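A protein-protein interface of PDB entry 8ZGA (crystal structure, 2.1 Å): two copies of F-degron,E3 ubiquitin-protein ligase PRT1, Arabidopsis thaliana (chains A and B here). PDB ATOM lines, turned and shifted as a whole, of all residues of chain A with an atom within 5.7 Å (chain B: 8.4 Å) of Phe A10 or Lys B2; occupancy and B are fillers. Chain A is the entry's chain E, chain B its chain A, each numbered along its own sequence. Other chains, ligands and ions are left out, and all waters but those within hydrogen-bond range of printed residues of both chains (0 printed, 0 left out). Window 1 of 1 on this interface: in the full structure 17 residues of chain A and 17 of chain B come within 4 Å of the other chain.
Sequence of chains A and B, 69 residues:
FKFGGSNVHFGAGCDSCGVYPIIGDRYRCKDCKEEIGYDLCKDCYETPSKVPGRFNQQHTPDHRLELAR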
ATOM      1  N   LYS A   2      -8.167 -13.906   1.594  1.00  0.00           N
ATOM      2  CA  LYS A   2      -8.037 -15.144   0.832  1.00  0.00           C
ATOM      3  C   LYS A   2      -6.856 -15.920   1.384  1.00  0.00           C
ATOM      4  O   LYS A   2      -5.712 -15.466   1.288  1.00  0.00           O
ATOM      5  CB  LYS A   2      -7.855 -14.881  -0.661  1.00  0.00           C
ATOM      6  CG  LYS A   2      -7.864 -16.148  -1.500  1.00  0.00           C
ATOM      7  CD  LYS A   2      -6.871 -16.123  -2.664  1.00  0.00           C
ATOM      8  CE  LYS A   2      -6.774 -17.528  -3.281  1.00  0.00           C
ATOM      9  NZ  LYS A   2      -6.132 -18.535  -2.376  1.00  0.00           N
ATOM     10  N   PHE A   3      -7.142 -17.096   1.935  1.00  0.00           N
ATOM     11  CA  PHE A   3      -6.102 -17.946   2.490  1.00  0.00           C
ATOM     12  C   PHE A   3      -5.216 -18.488   1.378  1.00  0.00           C
ATOM     13  O   PHE A   3      -5.709 -18.958   0.348  1.00  0.00           O
ATOM     14  CB  PHE A   3      -6.730 -19.088   3.288  1.00  0.00           C
ATOM     15  CG  PHE A   3      -7.597 -18.614   4.416  1.00  0.00           C
ATOM     16  CD1 PHE A   3      -7.034 -17.994   5.516  1.00  0.00           C
ATOM     17  CD2 PHE A   3      -8.971 -18.787   4.379  1.00  0.00           C
ATOM     18  CE1 PHE A   3      -7.823 -17.545   6.556  1.00  0.00           C
ATOM     19  CE2 PHE A   3      -9.767 -18.343   5.419  1.00  0.00           C
ATOM     20  CZ  PHE A   3      -9.191 -17.720   6.510  1.00  0.00           C
ATOM     21  N   GLY A   4      -3.903 -18.435   1.599  1.00  0.00           N
ATOM     22  CA  GLY A   4      -2.931 -18.883   0.629  1.00  0.00           C
ATOM     23  C   GLY A   4      -2.474 -17.827  -0.355  1.00  0.00           C
ATOM     24  O   GLY A   4      -1.435 -18.010  -1.000  1.00  0.00           O
ATOM     25  N   VAL A   8      -1.934 -20.654  -4.017  1.00  0.00           N
ATOM     26  CA  VAL A   8      -2.880 -21.740  -4.248  1.00  0.00           C
ATOM     27  C   VAL A   8      -4.132 -21.147  -4.873  1.00  0.00           C
ATOM     28  O   VAL A   8      -4.547 -20.041  -4.516  1.00  0.00           O
ATOM     29  CB  VAL A   8      -3.218 -22.492  -2.942  1.00  0.00           C
ATOM     30  CG1 VAL A   8      -3.868 -21.544  -1.927  1.00  0.00           C
ATOM     31  CG2 VAL A   8      -4.134 -23.677  -3.214  1.00  0.00           C
ATOM     32  N   HIS A   9      -4.745 -21.886  -5.796  1.00  0.00           N
ATOM     33  CA  HIS A   9      -5.941 -21.435  -6.507  1.00  0.00           C
ATOM     34  C   HIS A   9      -6.970 -22.554  -6.390  1.00  0.00           C
ATOM     35  O   HIS A   9      -7.043 -23.438  -7.247  1.00  0.00           O
ATOM     36  CB  HIS A   9      -5.617 -21.092  -7.953  1.00  0.00           C
ATOM     37  CG  HIS A   9      -4.566 -20.035  -8.098  1.00  0.00           C
ATOM     38  ND1 HIS A   9      -3.224 -20.290  -7.917  1.00  0.00           N
ATOM     39  CD2 HIS A   9      -4.661 -18.719  -8.402  1.00  0.00           C
ATOM     40  CE1 HIS A   9      -2.537 -19.176  -8.109  1.00  0.00           C
ATOM     41  NE2 HIS A   9      -3.386 -18.209  -8.402  1.00  0.00           N
ATOM     42  N   PHE A  10      -7.752 -22.516  -5.315  1.00  0.00           N
ATOM     43  CA  PHE A  10      -8.754 -23.544  -5.087  1.00  0.00           C
ATOM     44  C   PHE A  10      -9.786 -23.530  -6.205  1.00  0.00           C
ATOM     45  O   PHE A  10     -10.151 -22.471  -6.726  1.00  0.00           O
ATOM     46  CB  PHE A  10      -9.434 -23.328  -3.736  1.00  0.00           C
ATOM     47  CG  PHE A  10      -8.474 -23.251  -2.587  1.00  0.00           C
ATOM     48  CD1 PHE A  10      -7.816 -24.385  -2.143  1.00  0.00           C
ATOM     49  CD2 PHE A  10      -8.227 -22.046  -1.949  1.00  0.00           C
ATOM     50  CE1 PHE A  10      -6.930 -24.321  -1.088  1.00  0.00           C
ATOM     51  CE2 PHE A  10      -7.342 -21.975  -0.892  1.00  0.00           C
ATOM     52  CZ  PHE A  10      -6.692 -23.114  -0.461  1.00  0.00           C
ATOM     53  N   GLY A  11     -10.255 -24.717  -6.575  1.00  0.00           N
ATOM     54  CA  GLY A  11     -11.226 -24.854  -7.635  1.00  0.00           C
ATOM     55  C   GLY A  11     -10.689 -24.639  -9.030  1.00  0.00           C
ATOM     56  O   GLY A  11     -11.463 -24.735  -9.989  1.00  0.00           O
ATOM     57  N   ALA A  12      -9.397 -24.358  -9.178  1.00  0.00           N
ATOM     58  CA  ALA A  12      -8.779 -24.121 -10.476  1.00  0.00           C
ATOM     59  C   ALA A  12      -7.841 -25.275 -10.802  1.00  0.00           C
ATOM     60  O   ALA A  12      -7.064 -25.709  -9.945  1.00  0.00           O
ATOM     61  CB  ALA A  12      -8.015 -22.795 -10.485  1.00  0.00           C
ATOM     62  N   GLY A  13      -7.916 -25.770 -12.040  1.00  0.00           N
ATOM     63  CA  GLY A  13      -7.080 -26.869 -12.470  1.00  0.00           C
ATOM     64  C   GLY A  13      -6.403 -26.562 -13.789  1.00  0.00           C
ATOM     65  O   GLY A  13      -6.896 -25.782 -14.602  1.00  0.00           O
ATOM     66  N   TYR A  20      -4.917 -30.282  -9.719  1.00  0.00           N
ATOM     67  CA  TYR A  20      -6.056 -29.595  -9.122  1.00  0.00           C
ATOM     68  C   TYR A  20      -6.033 -29.734  -7.603  1.00  0.00           C
ATOM     69  O   TYR A  20      -6.109 -30.856  -7.088  1.00  0.00           O
ATOM     70  CB  TYR A  20      -7.366 -30.157  -9.682  1.00  0.00           C
ATOM     71  CG  TYR A  20      -8.612 -29.563  -9.065  1.00  0.00           C
ATOM     72  CD1 TYR A  20      -9.136 -30.073  -7.886  1.00  0.00           C
ATOM     73  CD2 TYR A  20      -9.267 -28.494  -9.661  1.00  0.00           C
ATOM     74  CE1 TYR A  20     -10.270 -29.534  -7.312  1.00  0.00           C
ATOM     75  CE2 TYR A  20     -10.405 -27.947  -9.093  1.00  0.00           C
ATOM     76  CZ  TYR A  20     -10.901 -28.474  -7.919  1.00  0.00           C
ATOM     77  OH  TYR A  20     -12.034 -27.940  -7.351  1.00  0.00           O
ATOM     78  N   PRO A  21      -5.948 -28.625  -6.846  1.00  0.00           N
ATOM     79  CA  PRO A  21      -5.869 -27.237  -7.327  1.00  0.00           C
ATOM     80  C   PRO A  21      -4.474 -26.858  -7.822  1.00  0.00           C
ATOM     81  O   PRO A  21      -3.508 -27.554  -7.513  1.00  0.00           O
ATOM     82  CB  PRO A  21      -6.247 -26.419  -6.092  1.00  0.00           C
ATOM     83  CG  PRO A  21      -5.772 -27.251  -4.945  1.00  0.00           C
ATOM     84  CD  PRO A  21      -5.940 -28.699  -5.372  1.00  0.00           C
ATOM     85  N   ILE A  22      -4.370 -25.770  -8.582  1.00  0.00           N
ATOM     86  CA  ILE A  22      -3.066 -25.305  -9.039  1.00  0.00           C
ATOM     87  C   ILE A  22      -2.307 -24.729  -7.851  1.00  0.00           C
ATOM     88  O   ILE A  22      -2.776 -23.798  -7.188  1.00  0.00           O
ATOM     89  CB  ILE A  22      -3.210 -24.271 -10.165  1.00  0.00           C
ATOM     90  CG1 ILE A  22      -3.846 -24.926 -11.394  1.00  0.00           C
ATOM     91  CG2 ILE A  22      -1.852 -23.670 -10.510  1.00  0.00           C
ATOM     92  CD1 ILE A  22      -4.015 -24.002 -12.583  1.00  0.00           C
ATOM     93  N   ARG A  26      -0.585 -19.248 -11.457  1.00  0.00           N
ATOM     94  CA  ARG A  26      -1.614 -19.694 -12.382  1.00  0.00           C
ATOM     95  C   ARG A  26      -1.739 -18.686 -13.513  1.00  0.00           C
ATOM     96  O   ARG A  26      -1.674 -17.473 -13.288  1.00  0.00           O
ATOM     97  CB  ARG A  26      -2.948 -19.865 -11.656  1.00  0.00           C
ATOM     98  CG  ARG A  26      -4.168 -19.917 -12.566  1.00  0.00           C
ATOM     99  CD  ARG A  26      -5.441 -19.734 -11.758  1.00  0.00           C
ATOM    100  NE  ARG A  26      -6.629 -19.550 -12.585  1.00  0.00           N
ATOM    101  CZ  ARG A  26      -7.784 -19.101 -12.107  1.00  0.00           C
ATOM    102  NH1 ARG A  26      -7.885 -18.785 -10.824  1.00  0.00           N
ATOM    103  NH2 ARG A  26      -8.835 -18.957 -12.897  1.00  0.00           N
ATOM    104  N   GLU A  35     -17.455 -20.724 -19.708  1.00  0.00           N
ATOM    105  CA  GLU A  35     -17.447 -20.276 -18.320  1.00  0.00           C
ATOM    106  C   GLU A  35     -16.516 -21.126 -17.470  1.00  0.00           C
ATOM    107  O   GLU A  35     -16.009 -20.654 -16.446  1.00  0.00           O
ATOM    108  CB  GLU A  35     -18.867 -20.299 -17.755  1.00  0.00           C
ATOM    109  CG  GLU A  35     -19.032 -19.560 -16.440  1.00  0.00           C
ATOM    110  CD  GLU A  35     -20.487 -19.268 -16.125  1.00  0.00           C
ATOM    111  OE1 GLU A  35     -21.369 -19.703 -16.897  1.00  0.00           O
ATOM    112  OE2 GLU A  35     -20.746 -18.598 -15.106  1.00  0.00           O
ATOM    113  N   ILE A  36     -16.275 -22.374 -17.876  1.00  0.00           N
ATOM    114  CA  ILE A  36     -15.306 -23.202 -17.167  1.00  0.00           C
ATOM    115  C   ILE A  36     -13.916 -22.594 -17.267  1.00  0.00           C
ATOM    116  O   ILE A  36     -13.077 -22.786 -16.379  1.00  0.00           O
ATOM    117  CB  ILE A  36     -15.336 -24.640 -17.720  1.00  0.00           C
ATOM    118  CG1 ILE A  36     -14.437 -25.549 -16.883  1.00  0.00           C
ATOM    119  CG2 ILE A  36     -14.887 -24.661 -19.172  1.00  0.00           C
ATOM    120  CD1 ILE A  36     -14.895 -25.717 -15.449  1.00  0.00           C
ATOM    121  N   GLY A  37     -13.649 -21.853 -18.338  1.00  0.00           N
ATOM    122  CA  GLY A  37     -12.380 -21.179 -18.499  1.00  0.00           C
ATOM    123  C   GLY A  37     -11.268 -22.106 -18.944  1.00  0.00           C
ATOM    124  O   GLY A  37     -11.432 -23.316 -19.112  1.00  0.00           O
ATOM    125  N   ASP A  39      -7.074 -22.632 -17.973  1.00  0.00           N
ATOM    126  CA  ASP A  39      -6.020 -22.265 -17.041  1.00  0.00           C
ATOM    127  C   ASP A  39      -4.816 -23.169 -17.256  1.00  0.00           C
ATOM    128  O   ASP A  39      -4.934 -24.291 -17.749  1.00  0.00           O
ATOM    129  CB  ASP A  39      -6.493 -22.364 -15.582  1.00  0.00           C
ATOM    130  CG  ASP A  39      -7.693 -21.485 -15.298  1.00  0.00           C
ATOM    131  OD1 ASP A  39      -8.823 -21.897 -15.630  1.00  0.00           O
ATOM    132  OD2 ASP A  39      -7.502 -20.380 -14.747  1.00  0.00           O
ATOM    133  N   PHE B   1      -9.029 -24.858 -15.904  1.00  0.00           N
ATOM    134  CA  PHE B   1     -10.471 -24.839 -15.669  1.00  0.00           C
ATOM    135  C   PHE B   1     -10.784 -24.424 -14.238  1.00  0.00           C
ATOM    136  O   PHE B   1     -10.026 -24.735 -13.331  1.00  0.00           O
ATOM    137  CB  PHE B   1     -11.070 -26.219 -15.978  1.00  0.00           C
ATOM    138  CG  PHE B   1     -10.372 -27.358 -15.283  1.00  0.00           C
ATOM    139  CD1 PHE B   1      -9.317 -28.022 -15.888  1.00  0.00           C
ATOM    140  CD2 PHE B   1     -10.785 -27.775 -14.031  1.00  0.00           C
ATOM    141  CE1 PHE B   1      -8.675 -29.071 -15.247  1.00  0.00           C
ATOM    142  CE2 PHE B   1     -10.147 -28.825 -13.381  1.00  0.00           C
ATOM    143  CZ  PHE B   1      -9.089 -29.472 -13.992  1.00  0.00           C
ATOM    144  N   LYS B   2     -11.888 -23.699 -14.055  1.00  0.00           N
ATOM    145  CA  LYS B   2     -12.323 -23.232 -12.740  1.00  0.00           C
ATOM    146  C   LYS B   2     -13.813 -23.501 -12.601  1.00  0.00           C
ATOM    147  O   LYS B   2     -14.621 -22.909 -13.323  1.00  0.00           O
ATOM    148  CB  LYS B   2     -12.025 -21.743 -12.560  1.00  0.00           C
ATOM    149  CG  LYS B   2     -12.774 -21.063 -11.414  1.00  0.00           C
ATOM    150  CD  LYS B   2     -12.447 -21.676 -10.063  1.00  0.00           C
ATOM    151  CE  LYS B   2     -13.034 -20.841  -8.923  1.00  0.00           C
ATOM    152  NZ  LYS B   2     -14.503 -20.612  -9.074  1.00  0.00           N
ATOM    153  N   PHE B   3     -14.175 -24.357 -11.646  1.00  0.00           N
ATOM    154  CA  PHE B   3     -15.572 -24.714 -11.434  1.00  0.00           C
ATOM    155  C   PHE B   3     -16.313 -23.601 -10.704  1.00  0.00           C
ATOM    156  O   PHE B   3     -15.784 -22.993  -9.766  1.00  0.00           O
ATOM    157  CB  PHE B   3     -15.676 -26.034 -10.653  1.00  0.00           C
ATOM    158  CG  PHE B   3     -14.950 -27.174 -11.313  1.00  0.00           C
ATOM    159  CD1 PHE B   3     -15.389 -27.676 -12.528  1.00  0.00           C
ATOM    160  CD2 PHE B   3     -13.816 -27.724 -10.739  1.00  0.00           C
ATOM    161  CE1 PHE B   3     -14.708 -28.708 -13.156  1.00  0.00           C
ATOM    162  CE2 PHE B   3     -13.138 -28.755 -11.368  1.00  0.00           C
ATOM    163  CZ  PHE B   3     -13.584 -29.244 -12.572  1.00  0.00           C
ATOM    164  N   GLY B   4     -17.558 -23.351 -11.130  1.00  0.00           N
ATOM    165  CA  GLY B   4     -18.367 -22.283 -10.585  1.00  0.00           C
ATOM    166  C   GLY B   4     -18.125 -20.923 -11.202  1.00  0.00           C
ATOM    167  O   GLY B   4     -18.944 -20.016 -11.012  1.00  0.00           O
ATOM    168  N   GLY B   5     -17.013 -20.747 -11.908  1.00  0.00           N
ATOM    169  CA  GLY B   5     -16.747 -19.471 -12.539  1.00  0.00           C
ATOM    170  C   GLY B   5     -16.617 -18.368 -11.512  1.00  0.00           C
ATOM    171  O   GLY B   5     -15.984 -18.524 -10.461  1.00  0.00           O
ATOM    172  N   SER B   6     -17.230 -17.232 -11.821  1.00  0.00           N
ATOM    173  CA  SER B   6     -17.229 -16.079 -10.934  1.00  0.00           C
ATOM    174  C   SER B   6     -18.376 -16.102  -9.928  1.00  0.00           C
ATOM    175  O   SER B   6     -18.583 -15.109  -9.220  1.00  0.00           O
ATOM    176  CB  SER B   6     -17.284 -14.795 -11.760  1.00  0.00           C
ATOM    177  OG  SER B   6     -18.454 -14.767 -12.554  1.00  0.00           O
ATOM    178  N   ASN B   7     -19.101 -17.216  -9.826  1.00  0.00           N
ATOM    179  CA  ASN B   7     -20.211 -17.344  -8.889  1.00  0.00           C
ATOM    180  C   ASN B   7     -19.784 -17.846  -7.517  1.00  0.00           C
ATOM    181  O   ASN B   7     -20.586 -17.785  -6.575  1.00  0.00           O
ATOM    182  CB  ASN B   7     -21.278 -18.283  -9.469  1.00  0.00           C
ATOM    183  CG  ASN B   7     -22.107 -17.620 -10.546  1.00  0.00           C
ATOM    184  OD1 ASN B   7     -22.442 -16.440 -10.445  1.00  0.00           O
ATOM    185  ND2 ASN B   7     -22.460 -18.378 -11.575  1.00  0.00           N
ATOM    186  N   VAL B   8     -18.553 -18.335  -7.389  1.00  0.00           N
ATOM    187  CA  VAL B   8     -17.997 -18.788  -6.116  1.00  0.00           C
ATOM    188  C   VAL B   8     -16.513 -18.466  -6.132  1.00  0.00           C
ATOM    189  O   VAL B   8     -15.871 -18.525  -7.183  1.00  0.00           O
ATOM    190  CB  VAL B   8     -18.239 -20.297  -5.882  1.00  0.00           C
ATOM    191  CG1 VAL B   8     -17.577 -21.117  -6.984  1.00  0.00           C
ATOM    192  CG2 VAL B   8     -17.718 -20.730  -4.511  1.00  0.00           C
ATOM    193  N   HIS B   9     -15.967 -18.121  -4.969  1.00  0.00           N
ATOM    194  CA  HIS B   9     -14.567 -17.726  -4.843  1.00  0.00           C
ATOM    195  C   HIS B   9     -14.005 -18.528  -3.677  1.00  0.00           C
ATOM    196  O   HIS B   9     -13.996 -18.072  -2.530  1.00  0.00           O
ATOM    197  CB  HIS B   9     -14.448 -16.225  -4.647  1.00  0.00           C
ATOM    198  CG  HIS B   9     -15.152 -15.431  -5.704  1.00  0.00           C
ATOM    199  ND1 HIS B   9     -14.500 -14.897  -6.794  1.00  0.00           N
ATOM    200  CD2 HIS B   9     -16.455 -15.091  -5.843  1.00  0.00           C
ATOM    201  CE1 HIS B   9     -15.369 -14.255  -7.554  1.00  0.00           C
ATOM    202  NE2 HIS B   9     -16.563 -14.358  -6.999  1.00  0.00           N
ATOM    203  N   PHE B  10     -13.555 -19.743  -3.981  1.00  0.00           N
ATOM    204  CA  PHE B  10     -13.031 -20.621  -2.951  1.00  0.00           C
ATOM    205  C   PHE B  10     -11.793 -20.004  -2.317  1.00  0.00           C
ATOM    206  O   PHE B  10     -10.961 -19.395  -2.996  1.00  0.00           O
ATOM    207  CB  PHE B  10     -12.697 -21.989  -3.543  1.00  0.00           C
ATOM    208  CG  PHE B  10     -13.866 -22.658  -4.205  1.00  0.00           C
ATOM    209  CD1 PHE B  10     -14.917 -23.148  -3.448  1.00  0.00           C
ATOM    210  CD2 PHE B  10     -13.915 -22.796  -5.581  1.00  0.00           C
ATOM    211  CE1 PHE B  10     -15.997 -23.761  -4.053  1.00  0.00           C
ATOM    212  CE2 PHE B  10     -14.989 -23.412  -6.191  1.00  0.00           C
ATOM    213  CZ  PHE B  10     -16.032 -23.895  -5.426  1.00  0.00           C
ATOM    214  N   GLY B  11     -11.676 -20.172  -1.005  1.00  0.00           N
ATOM    215  CA  GLY B  11     -10.578 -19.608  -0.263  1.00  0.00           C
ATOM    216  C   GLY B  11     -10.689 -18.129   0.015  1.00  0.00           C
ATOM    217  O   GLY B  11      -9.821 -17.587   0.707  1.00  0.00           O
ATOM    218  N   ALA B  12     -11.727 -17.462  -0.484  1.00  0.00           N
ATOM    219  CA  ALA B  12     -11.911 -16.027  -0.311  1.00  0.00           C
ATOM    220  C   ALA B  12     -13.089 -15.771   0.618  1.00  0.00           C
ATOM    221  O   ALA B  12     -14.151 -16.386   0.466  1.00  0.00           O
ATOM    222  CB  ALA B  12     -12.145 -15.338  -1.658  1.00  0.00           C
ATOM    223  N   TYR B  20     -17.599 -17.291   4.079  1.00  0.00           N
ATOM    224  CA  TYR B  20     -16.501 -18.045   3.486  1.00  0.00           C
ATOM    225  C   TYR B  20     -16.996 -19.414   3.024  1.00  0.00           C
ATOM    226  O   TYR B  20     -17.516 -20.185   3.843  1.00  0.00           O
ATOM    227  CB  TYR B  20     -15.364 -18.192   4.502  1.00  0.00           C
ATOM    228  CG  TYR B  20     -14.167 -18.952   3.982  1.00  0.00           C
ATOM    229  CD1 TYR B  20     -14.128 -20.336   4.032  1.00  0.00           C
ATOM    230  CD2 TYR B  20     -13.079 -18.285   3.431  1.00  0.00           C
ATOM    231  CE1 TYR B  20     -13.042 -21.040   3.550  1.00  0.00           C
ATOM    232  CE2 TYR B  20     -11.985 -18.982   2.946  1.00  0.00           C
ATOM    233  CZ  TYR B  20     -11.973 -20.358   3.008  1.00  0.00           C
ATOM    234  OH  TYR B  20     -10.887 -21.054   2.527  1.00  0.00           O
ATOM    235  N   PRO B  21     -16.894 -19.748   1.721  1.00  0.00           N
ATOM    236  CA  PRO B  21     -16.382 -18.871   0.657  1.00  0.00           C
ATOM    237  C   PRO B  21     -17.366 -17.780   0.221  1.00  0.00           C
ATOM    238  O   PRO B  21     -18.553 -17.902   0.509  1.00  0.00           O
ATOM    239  CB  PRO B  21     -16.132 -19.842  -0.497  1.00  0.00           C
ATOM    240  CG  PRO B  21     -17.157 -20.906  -0.307  1.00  0.00           C
ATOM    241  CD  PRO B  21     -17.324 -21.059   1.190  1.00  0.00           C
ATOM    242  N   ILE B  22     -16.892 -16.749  -0.481  1.00  0.00           N
ATOM    243  CA  ILE B  22     -17.789 -15.712  -0.984  1.00  0.00           C
ATOM    244  C   ILE B  22     -18.624 -16.295  -2.116  1.00  0.00           C
ATOM    245  O   ILE B  22     -18.086 -16.819  -3.099  1.00  0.00           O
ATOM    246  CB  ILE B  22     -17.005 -14.474  -1.449  1.00  0.00           C
ATOM    247  CG1 ILE B  22     -16.326 -13.805  -0.249  1.00  0.00           C
ATOM    248  CG2 ILE B  22     -17.928 -13.491  -2.166  1.00  0.00           C
ATOM    249  CD1 ILE B  22     -15.518 -12.571  -0.581  1.00  0.00           C
ATOM    250  N   ARG B  26     -17.436 -10.738  -6.054  1.00  0.00           N
ATOM    251  CA  ARG B  26     -16.403 -10.482  -5.063  1.00  0.00           C
ATOM    252  C   ARG B  26     -15.601  -9.262  -5.487  1.00  0.00           C
ATOM    253  O   ARG B  26     -15.347  -9.062  -6.679  1.00  0.00           O
ATOM    254  CB  ARG B  26     -15.499 -11.707  -4.927  1.00  0.00           C
ATOM    255  CG  ARG B  26     -14.192 -11.493  -4.185  1.00  0.00           C
ATOM    256  CD  ARG B  26     -13.188 -12.529  -4.638  1.00  0.00           C
ATOM    257  NE  ARG B  26     -11.897 -12.411  -3.977  1.00  0.00           N
ATOM    258  CZ  ARG B  26     -10.782 -12.952  -4.455  1.00  0.00           C
ATOM    259  NH1 ARG B  26     -10.814 -13.624  -5.596  1.00  0.00           N
ATOM    260  NH2 ARG B  26      -9.639 -12.817  -3.807  1.00  0.00           N
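The backbone NH (N) of Phe B1 is in hydrogen-bond range of the backbone carbonyl oxygen (O) of Gly A13 (2.7 Å).
The backbone NH (N) of Phe B1 lies within hydrogen-bond range of the side-chain carboxylate (OD1) of Asp A39 (3.0 Å).
The backbone NH of Lys B2 lies within hydrogen-bond range of the backbone carbonyl oxygen of Ile A36 (2.8 Å).
The backbone NH (N) of Phe B3 is in hydrogen-bond range of the backbone carbonyl oxygen (O) of Gly A11, 3.2 Å away.
The backbone NH (N) of Phe A3 lies within hydrogen-bond range of the backbone carbonyl oxygen (O) of Gly B11, at 3.0 Å.
The side-chain amino group of Lys B2 sits at hydrogen-bond distance from the backbone carbonyl oxygen of Gly B5, at 2.9 Å.
The side-chain amino group (NZ) of Lys B2 sits at hydrogen-bond distance from the backbone carbonyl oxygen (O) of Val B8, 3.1 Å away.
NZ of Lys A2 is in hydrogen-bond range of O of Val A8, 3.1 Å away.
O of Ala A12 lies within hydrogen-bond range of N of Ile A22 (3.0 Å).
OD2 of Asp A39 is in salt-bridge range of NE of Arg A26 (2.5 Å).
Among the printed residues, merely in contact across the chains: Lys A2 with Gly B11 (3.0 Å), Ala A12 with Phe B1 (3.2 Å), Gly A11 with Lys B2 (3.2 Å), Phe A3 with Tyr B20 (3.3 Å), Ile A36 with Phe B1 (3.4 Å), Phe A10 with Phe B10 (3.5 Å), Ile A36 with Phe B3 (3.6 Å), Gly A11 with Phe B1 (3.6 Å), Tyr A20 with Phe B3 (3.6 Å), Phe A10 with Gly B11 (3.8 Å), Tyr A20 with Phe B1 (3.8 Å), Gly A37 with Phe B1 (3.9 Å), Asp A39 with Lys B2 (3.9 Å), Glu A35 with Asn B7 (3.9 Å), Gly A11 with Phe B10 (3.96 Å) and Phe A10 with Lys B2 (3.97 Å).
Of the printed residues of chain B, Phe A10 touches Lys B2, Phe B10 and Gly B11.
Lys B2 touches four residues of chain A.
Printed residues of chain B within 4 Å of Gly A11: Phe B1, Lys B2, Phe B3 and Phe B10.
Of the printed residues of chain A, Phe B10 touches Phe A10 (3.5 Å) and Gly A11 (3.96 Å).
Of the printed residues of chain B, Tyr A20 touches Phe B1 (3.8 Å) and Phe B3 (3.6 Å).
Printed residues of chain B within 4 Å of Glu A35: Asn B7.
Of the printed residues of chain A, Gly B11 touches Lys A2, Phe A3 and Phe A10.
The nearest residue of chain B that does not touch Phe A10 is Tyr B20 (5.0 Å).
The nearest printed residue of chain B that does not touch Glu A35 is Lys B2 (4.1 Å).
Of the 16 printed residues of chain B, 7 touch a printed residue of chain A.
Printed residues of chain B that touch a printed residue of chain A: Phe B1, Lys B2, Phe B3, Asn B7, Phe B10, Gly B11 and Tyr B20.
Hydrophobic or aromatic side chains of chain B that line the printed part of chain A: Phe B1, Phe B3, Phe B10 and Tyr B20.
Of the 17 printed residues of chain A, 11 touch a printed residue of chain B.
Printed residues of chain A that touch a printed residue of chain B: Lys A2, Phe A3, Phe A10, Gly A11, Ala A12, Gly A13, Tyr A20, Glu A35, Ile A36, Gly A37 and Asp A39.
Hydrophobic or aromatic side chains of chain A that line the printed part of chain B: Phe A3, Phe A10, Ala A12, Tyr A20 and Ile A36.
Among the printed residues, 21 pairs touch across the chains.
Lys A2 touches Gly B11, and with the chains exchanged Gly A11 touches Lys B2.
Phe A3 touches Tyr B20, and with the chains exchanged Tyr A20 touches Phe B3.
Phe B10 touches its own counterpart, Phe A10.
Phe A10 touches Gly B11, and with the chains exchanged Gly A11 touches Phe B10.
12 positions are printed for both chains.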
